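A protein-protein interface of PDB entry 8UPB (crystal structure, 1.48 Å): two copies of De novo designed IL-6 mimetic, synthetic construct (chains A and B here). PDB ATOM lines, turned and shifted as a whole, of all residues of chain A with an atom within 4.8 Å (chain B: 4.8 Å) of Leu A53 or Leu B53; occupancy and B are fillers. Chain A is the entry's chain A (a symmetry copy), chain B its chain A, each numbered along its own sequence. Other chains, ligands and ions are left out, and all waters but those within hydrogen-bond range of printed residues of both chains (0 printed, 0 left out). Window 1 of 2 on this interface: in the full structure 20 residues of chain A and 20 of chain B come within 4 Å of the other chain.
Of the 11 printed residues of chain A, 7 touch a printed residue of chain B.
Printed residues of chain B that touch a printed residue of chain A: Phe B12, Val B16, Leu B49, Leu B50, Leu B52, Leu B53 and Ile B56.
Hydrophobic or aromatic side chains of chain B that line the printed part of chain A: Phe B12, Val B16, Leu B49, Leu B50, Leu B52, Leu B53 and Ile B56.
Among the printed residues, 12 pairs touch across the chains.
Val A16 touches Leu B52, and with the chains exchanged Leu A52 touches Val B16.
Val A16 touches Ile B56, and with the chains exchanged Ile A56 touches Val B16.
Leu A49 touches Leu B53, and with the chains exchanged Leu A53 touches Leu B49.
Leu B53 touches its own counterpart, Leu A53.
Positions printed for both chains: 12, 16, 49, 50, 51, 52, 53, 54, 55, 56 and 57.
Of the printed residues of chain B, Leu A53 touches Leu B49 (3.97 Å) and Leu B53 (3.98 Å).
Of the printed residues of chain B, Leu A50 touches Leu B49 (3.8 Å).
Of the printed residues of chain B, Leu A49 touches Phe B12, Leu B50 and Leu B53.
Of the printed residues of chain B, Phe A12 touches Leu B49 (3.96 Å).
Of the printed residues of chain B, Ile A56 touches Val B16 and Ile B56.
Of the printed residues of chain B, Val A16 touches Leu B52 (3.9 Å) and Ile B56 (3.8 Å).
Phe A12 touches Leu B49.
Leu B52 touches Val A16.
Ile B56 touches Val A16 (CD1 to CG1, 3.8 Å).
Leu A49 touches Phe B12 (CD1 to CD2, 3.96 Å).
CD2 of Leu A49 touches CD1 of Leu B50, at 3.8 Å.
Leu A49 touches Leu B53 (CD1 to CD1, 3.97 Å).
CD2 of Leu B49 touches CD1 of Leu A50 (3.8 Å).
Leu A52 touches Val B16 (CB to CG1, 3.9 Å).
Leu A53 touches Leu B53 (CB to CD1, 3.98 Å).
Val B16 touches Ile A56.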
ATOM      1  N   PHE A  12     -22.565   1.910 -22.859  1.00  0.00           N
ATOM      2  CA  PHE A  12     -22.235   0.785 -21.990  1.00  0.00           C
ATOM      3  C   PHE A  12     -20.734   0.508 -21.990  1.00  0.00           C
ATOM      4  O   PHE A  12     -20.130   0.321 -20.930  1.00  0.00           O
ATOM      5  CB  PHE A  12     -22.996  -0.464 -22.432  1.00  0.00           C
ATOM      6  CG  PHE A  12     -22.897  -1.617 -21.453  1.00  0.00           C
ATOM      7  CD1 PHE A  12     -23.768  -1.686 -20.377  1.00  0.00           C
ATOM      8  CD2 PHE A  12     -21.952  -2.632 -21.620  1.00  0.00           C
ATOM      9  CE1 PHE A  12     -23.716  -2.747 -19.456  1.00  0.00           C
ATOM     10  CE2 PHE A  12     -21.885  -3.690 -20.700  1.00  0.00           C
ATOM     11  CZ  PHE A  12     -22.784  -3.752 -19.623  1.00  0.00           C
ATOM     12  N   VAL A  16     -18.096   0.502 -18.891  1.00  0.00           N
ATOM     13  CA  VAL A  16     -17.271  -0.662 -18.570  1.00  0.00           C
ATOM     14  C   VAL A  16     -15.825  -0.244 -18.415  1.00  0.00           C
ATOM     15  O   VAL A  16     -15.135  -0.665 -17.481  1.00  0.00           O
ATOM     16  CB  VAL A  16     -17.438  -1.765 -19.629  1.00  0.00           C
ATOM     17  CG1 VAL A  16     -16.453  -2.910 -19.357  1.00  0.00           C
ATOM     18  CG2 VAL A  16     -18.885  -2.310 -19.624  1.00  0.00           C
ATOM     19  N   LEU A  49     -25.477 -10.408 -23.676  1.00  0.00           N
ATOM     20  CA  LEU A  49     -24.080 -10.336 -23.270  1.00  0.00           C
ATOM     21  C   LEU A  49     -23.851  -9.216 -22.269  1.00  0.00           C
ATOM     22  O   LEU A  49     -23.024  -9.351 -21.359  1.00  0.00           O
ATOM     23  CB  LEU A  49     -23.193 -10.119 -24.497  1.00  0.00           C
ATOM     24  CG  LEU A  49     -21.711 -10.262 -24.198  1.00  0.00           C
ATOM     25  CD1 LEU A  49     -21.417 -11.726 -23.859  1.00  0.00           C
ATOM     26  CD2 LEU A  49     -20.918  -9.774 -25.402  1.00  0.00           C
ATOM     27  N   LEU A  50     -24.565  -8.103 -22.421  1.00  0.00           N
ATOM     28  CA  LEU A  50     -24.398  -6.974 -21.512  1.00  0.00           C
ATOM     29  C   LEU A  50     -24.875  -7.333 -20.112  1.00  0.00           C
ATOM     30  O   LEU A  50     -24.257  -6.934 -19.117  1.00  0.00           O
ATOM     31  CB  LEU A  50     -25.134  -5.755 -22.055  1.00  0.00           C
ATOM     32  CG  LEU A  50     -24.326  -4.971 -23.102  1.00  0.00           C
ATOM     33  CD1 LEU A  50     -24.061  -5.763 -24.372  1.00  0.00           C
ATOM     34  CD2 LEU A  50     -25.017  -3.651 -23.419  1.00  0.00           C
ATOM     35  N   ARG A  51     -25.956  -8.110 -20.019  1.00  0.00           N
ATOM     36  CA  ARG A  51     -26.440  -8.575 -18.723  1.00  0.00           C
ATOM     37  C   ARG A  51     -25.449  -9.537 -18.084  1.00  0.00           C
ATOM     38  O   ARG A  51     -25.214  -9.489 -16.872  1.00  0.00           O
ATOM     39  CB  ARG A  51     -27.798  -9.271 -18.890  1.00  0.00           C
ATOM     40  CG  ARG A  51     -28.808  -8.463 -19.685  1.00  0.00           C
ATOM     41  CD  ARG A  51     -30.242  -8.880 -19.378  1.00  0.00           C
ATOM     42  NE  ARG A  51     -30.576 -10.162 -19.987  1.00  0.00           N
ATOM     43  CZ  ARG A  51     -30.954 -10.315 -21.249  1.00  0.00           C
ATOM     44  NH1 ARG A  51     -30.981  -9.296 -22.093  1.00  0.00           N
ATOM     45  NH2 ARG A  51     -31.321 -11.522 -21.674  1.00  0.00           N
ATOM     46  N   LEU A  52     -24.869 -10.428 -18.883  1.00  0.00           N
ATOM     47  CA  LEU A  52     -23.855 -11.337 -18.364  1.00  0.00           C
ATOM     48  C   LEU A  52     -22.610 -10.582 -17.912  1.00  0.00           C
ATOM     49  O   LEU A  52     -21.976 -10.972 -16.924  1.00  0.00           O
ATOM     50  CB  LEU A  52     -23.507 -12.373 -19.439  1.00  0.00           C
ATOM     51  CG  LEU A  52     -24.689 -13.261 -19.850  1.00  0.00           C
ATOM     52  CD1 LEU A  52     -24.292 -14.105 -21.051  1.00  0.00           C
ATOM     53  CD2 LEU A  52     -25.117 -14.135 -18.702  1.00  0.00           C
ATOM     54  N   LEU A  53     -22.219  -9.523 -18.639  1.00  0.00           N
ATOM     55  CA  LEU A  53     -21.077  -8.724 -18.197  1.00  0.00           C
ATOM     56  C   LEU A  53     -21.360  -8.098 -16.837  1.00  0.00           C
ATOM     57  O   LEU A  53     -20.500  -8.116 -15.949  1.00  0.00           O
ATOM     58  CB  LEU A  53     -20.735  -7.637 -19.224  1.00  0.00           C
ATOM     59  CG  LEU A  53     -19.386  -6.925 -19.006  1.00  0.00           C
ATOM     60  CD1 LEU A  53     -18.887  -6.401 -20.339  1.00  0.00           C
ATOM     61  CD2 LEU A  53     -19.517  -5.797 -17.978  1.00  0.00           C
ATOM     62  N   PHE A  54     -22.559  -7.546 -16.656  1.00  0.00           N
ATOM     63  CA  PHE A  54     -22.961  -7.041 -15.348  1.00  0.00           C
ATOM     64  C   PHE A  54     -22.810  -8.116 -14.276  1.00  0.00           C
ATOM     65  O   PHE A  54     -22.272  -7.859 -13.191  1.00  0.00           O
ATOM     66  CB  PHE A  54     -24.407  -6.544 -15.401  1.00  0.00           C
ATOM     67  CG  PHE A  54     -24.980  -6.242 -14.037  1.00  0.00           C
ATOM     68  CD1 PHE A  54     -24.858  -4.971 -13.484  1.00  0.00           C
ATOM     69  CD2 PHE A  54     -25.605  -7.232 -13.301  1.00  0.00           C
ATOM     70  CE1 PHE A  54     -25.365  -4.690 -12.211  1.00  0.00           C
ATOM     71  CE2 PHE A  54     -26.112  -6.955 -12.037  1.00  0.00           C
ATOM     72  CZ  PHE A  54     -25.999  -5.693 -11.498  1.00  0.00           C
ATOM     73  N   ARG A  55     -23.262  -9.335 -14.569  1.00  0.00           N
ATOM     74  CA  ARG A  55     -23.203 -10.390 -13.558  1.00  0.00           C
ATOM     75  C   ARG A  55     -21.776 -10.658 -13.107  1.00  0.00           C
ATOM     76  O   ARG A  55     -21.515 -10.834 -11.905  1.00  0.00           O
ATOM     77  CB  ARG A  55     -23.775 -11.672 -14.128  1.00  0.00           C
ATOM     78  CG  ARG A  55     -23.896 -12.809 -13.124  1.00  0.00           C
ATOM     79  CD  ARG A  55     -24.875 -13.717 -13.720  1.00  0.00           C
ATOM     80  NE  ARG A  55     -25.040 -15.031 -13.120  1.00  0.00           N
ATOM     81  CZ  ARG A  55     -25.936 -15.885 -13.587  1.00  0.00           C
ATOM     82  NH1 ARG A  55     -26.751 -15.543 -14.570  1.00  0.00           N
ATOM     83  NH2 ARG A  55     -26.010 -17.109 -13.070  1.00  0.00           N
ATOM     84  N   ILE A  56     -20.847 -10.734 -14.064  1.00  0.00           N
ATOM     85  CA  ILE A  56     -19.436 -10.958 -13.755  1.00  0.00           C
ATOM     86  C   ILE A  56     -18.870  -9.763 -13.002  1.00  0.00           C
ATOM     87  O   ILE A  56     -18.174  -9.920 -11.993  1.00  0.00           O
ATOM     88  CB  ILE A  56     -18.662 -11.242 -15.061  1.00  0.00           C
ATOM     89  CG1 ILE A  56     -19.168 -12.536 -15.708  1.00  0.00           C
ATOM     90  CG2 ILE A  56     -17.146 -11.260 -14.807  1.00  0.00           C
ATOM     91  CD1 ILE A  56     -18.654 -12.749 -17.132  1.00  0.00           C
ATOM     92  N   ALA A  57     -19.187  -8.556 -13.463  1.00  0.00           N
ATOM     93  CA  ALA A  57     -18.682  -7.348 -12.820  1.00  0.00           C
ATOM     94  C   ALA A  57     -19.169  -7.255 -11.379  1.00  0.00           C
ATOM     95  O   ALA A  57     -18.404  -6.881 -10.472  1.00  0.00           O
ATOM     96  CB  ALA A  57     -19.151  -6.119 -13.601  1.00  0.00           C
ATOM     97  N   PHE B  12     -19.182 -16.598 -28.357  1.00  0.00           N
ATOM     98  CA  PHE B  12     -18.634 -15.918 -27.189  1.00  0.00           C
ATOM     99  C   PHE B  12     -19.640 -15.892 -26.042  1.00  0.00           C
ATOM    100  O   PHE B  12     -19.291 -16.186 -24.894  1.00  0.00           O
ATOM    101  CB  PHE B  12     -18.221 -14.493 -27.554  1.00  0.00           C
ATOM    102  CG  PHE B  12     -17.429 -13.790 -26.468  1.00  0.00           C
ATOM    103  CD1 PHE B  12     -16.058 -13.974 -26.385  1.00  0.00           C
ATOM    104  CD2 PHE B  12     -18.051 -12.939 -25.553  1.00  0.00           C
ATOM    105  CE1 PHE B  12     -15.288 -13.329 -25.401  1.00  0.00           C
ATOM    106  CE2 PHE B  12     -17.292 -12.299 -24.560  1.00  0.00           C
ATOM    107  CZ  PHE B  12     -15.902 -12.485 -24.498  1.00  0.00           C
ATOM    108  N   VAL B  16     -19.313 -17.385 -22.270  1.00  0.00           N
ATOM    109  CA  VAL B  16     -19.487 -16.550 -21.081  1.00  0.00           C
ATOM    110  C   VAL B  16     -20.452 -17.212 -20.121  1.00  0.00           C
ATOM    111  O   VAL B  16     -20.217 -17.259 -18.910  1.00  0.00           O
ATOM    112  CB  VAL B  16     -19.943 -15.132 -21.465  1.00  0.00           C
ATOM    113  CG1 VAL B  16     -20.265 -14.322 -20.203  1.00  0.00           C
ATOM    114  CG2 VAL B  16     -18.846 -14.410 -22.281  1.00  0.00           C
ATOM    115  N   LEU B  49     -15.840  -4.497 -26.543  1.00  0.00           N
ATOM    116  CA  LEU B  49     -16.543  -4.921 -25.340  1.00  0.00           C
ATOM    117  C   LEU B  49     -16.174  -6.344 -24.954  1.00  0.00           C
ATOM    118  O   LEU B  49     -16.094  -6.667 -23.763  1.00  0.00           O
ATOM    119  CB  LEU B  49     -18.053  -4.823 -25.558  1.00  0.00           C
ATOM    120  CG  LEU B  49     -18.858  -5.023 -24.286  1.00  0.00           C
ATOM    121  CD1 LEU B  49     -18.602  -3.837 -23.352  1.00  0.00           C
ATOM    122  CD2 LEU B  49     -20.328  -5.168 -24.652  1.00  0.00           C
ATOM    123  N   LEU B  50     -15.951  -7.208 -25.942  1.00  0.00           N
ATOM    124  CA  LEU B  50     -15.604  -8.598 -25.660  1.00  0.00           C
ATOM    125  C   LEU B  50     -14.238  -8.688 -24.997  1.00  0.00           C
ATOM    126  O   LEU B  50     -14.034  -9.503 -24.088  1.00  0.00           O
ATOM    127  CB  LEU B  50     -15.657  -9.417 -26.943  1.00  0.00           C
ATOM    128  CG  LEU B  50     -17.072  -9.894 -27.306  1.00  0.00           C
ATOM    129  CD1 LEU B  50     -18.025  -8.754 -27.629  1.00  0.00           C
ATOM    130  CD2 LEU B  50     -17.013 -10.894 -28.453  1.00  0.00           C
ATOM    131  N   ARG B  51     -13.299  -7.839 -25.421  1.00  0.00           N
ATOM    132  CA  ARG B  51     -11.983  -7.794 -24.789  1.00  0.00           C
ATOM    133  C   ARG B  51     -12.082  -7.285 -23.359  1.00  0.00           C
ATOM    134  O   ARG B  51     -11.406  -7.794 -22.459  1.00  0.00           O
ATOM    135  CB  ARG B  51     -11.046  -6.886 -25.597  1.00  0.00           C
ATOM    136  CG  ARG B  51     -11.020  -7.197 -27.083  1.00  0.00           C
ATOM    137  CD  ARG B  51      -9.740  -6.701 -27.747  1.00  0.00           C
ATOM    138  NE  ARG B  51      -9.737  -5.252 -27.905  1.00  0.00           N
ATOM    139  CZ  ARG B  51     -10.333  -4.607 -28.900  1.00  0.00           C
ATOM    140  NH1 ARG B  51     -11.060  -5.244 -29.803  1.00  0.00           N
ATOM    141  NH2 ARG B  51     -10.189  -3.286 -28.993  1.00  0.00           N
ATOM    142  N   LEU B  52     -12.910  -6.268 -23.134  1.00  0.00           N
ATOM    143  CA  LEU B  52     -13.117  -5.768 -21.782  1.00  0.00           C
ATOM    144  C   LEU B  52     -13.785  -6.814 -20.897  1.00  0.00           C
ATOM    145  O   LEU B  52     -13.477  -6.901 -19.702  1.00  0.00           O
ATOM    146  CB  LEU B  52     -13.953  -4.485 -21.839  1.00  0.00           C
ATOM    147  CG  LEU B  52     -13.279  -3.339 -22.607  1.00  0.00           C
ATOM    148  CD1 LEU B  52     -14.268  -2.196 -22.777  1.00  0.00           C
ATOM    149  CD2 LEU B  52     -12.044  -2.874 -21.884  1.00  0.00           C
ATOM    150  N   LEU B  53     -14.728  -7.594 -21.450  1.00  0.00           N
ATOM    151  CA  LEU B  53     -15.337  -8.661 -20.659  1.00  0.00           C
ATOM    152  C   LEU B  53     -14.285  -9.678 -20.235  1.00  0.00           C
ATOM    153  O   LEU B  53     -14.261 -10.106 -19.075  1.00  0.00           O
ATOM    154  CB  LEU B  53     -16.461  -9.354 -21.443  1.00  0.00           C
ATOM    155  CG  LEU B  53     -17.359 -10.294 -20.615  1.00  0.00           C
ATOM    156  CD1 LEU B  53     -18.720 -10.382 -21.280  1.00  0.00           C
ATOM    157  CD2 LEU B  53     -16.721 -11.679 -20.468  1.00  0.00           C
ATOM    158  N   PHE B  54     -13.405 -10.067 -21.156  1.00  0.00           N
ATOM    159  CA  PHE B  54     -12.287 -10.935 -20.803  1.00  0.00           C
ATOM    160  C   PHE B  54     -11.478 -10.346 -19.651  1.00  0.00           C
ATOM    161  O   PHE B  54     -11.134 -11.049 -18.692  1.00  0.00           O
ATOM    162  CB  PHE B  54     -11.390 -11.154 -22.023  1.00  0.00           C
ATOM    163  CG  PHE B  54     -10.082 -11.828 -21.684  1.00  0.00           C
ATOM    164  CD1 PHE B  54      -9.974 -13.216 -21.704  1.00  0.00           C
ATOM    165  CD2 PHE B  54      -8.980 -11.080 -21.313  1.00  0.00           C
ATOM    166  CE1 PHE B  54      -8.773 -13.848 -21.368  1.00  0.00           C
ATOM    167  CE2 PHE B  54      -7.784 -11.705 -20.981  1.00  0.00           C
ATOM    168  CZ  PHE B  54      -7.679 -13.077 -21.013  1.00  0.00           C
ATOM    169  N   ARG B  55     -11.182  -9.048 -19.718  1.00  0.00           N
ATOM    170  CA  ARG B  55     -10.355  -8.441 -18.676  1.00  0.00           C
ATOM    171  C   ARG B  55     -10.995  -8.571 -17.302  1.00  0.00           C
ATOM    172  O   ARG B  55     -10.310  -8.874 -16.311  1.00  0.00           O
ATOM    173  CB  ARG B  55     -10.158  -6.969 -18.976  1.00  0.00           C
ATOM    174  CG  ARG B  55      -9.198  -6.257 -18.035  1.00  0.00           C
ATOM    175  CD  ARG B  55      -8.793  -5.058 -18.768  1.00  0.00           C
ATOM    176  NE  ARG B  55      -8.057  -4.033 -18.046  1.00  0.00           N
ATOM    177  CZ  ARG B  55      -7.628  -2.943 -18.661  1.00  0.00           C
ATOM    178  NH1 ARG B  55      -7.799  -2.787 -19.963  1.00  0.00           N
ATOM    179  NH2 ARG B  55      -7.028  -1.985 -17.959  1.00  0.00           N
ATOM    180  N   ILE B  56     -12.301  -8.304 -17.220  1.00  0.00           N
ATOM    181  CA  ILE B  56     -13.037  -8.422 -15.963  1.00  0.00           C
ATOM    182  C   ILE B  56     -13.087  -9.878 -15.522  1.00  0.00           C
ATOM    183  O   ILE B  56     -12.843 -10.196 -14.353  1.00  0.00           O
ATOM    184  CB  ILE B  56     -14.446  -7.816 -16.132  1.00  0.00           C
ATOM    185  CG1 ILE B  56     -14.348  -6.316 -16.430  1.00  0.00           C
ATOM    186  CG2 ILE B  56     -15.325  -8.120 -14.908  1.00  0.00           C
ATOM    187  CD1 ILE B  56     -15.671  -5.694 -16.879  1.00  0.00           C
ATOM    188  N   ALA B  57     -13.373 -10.780 -16.457  1.00  0.00           N
ATOM    189  CA  ALA B  57     -13.459 -12.200 -16.132  1.00  0.00           C
ATOM    190  C   ALA B  57     -12.127 -12.720 -15.610  1.00  0.00           C
ATOM    191  O   ALA B  57     -12.084 -13.503 -14.644  1.00  0.00           O
ATOM    192  CB  ALA B  57     -13.866 -12.986 -17.380  1.00  0.00           C
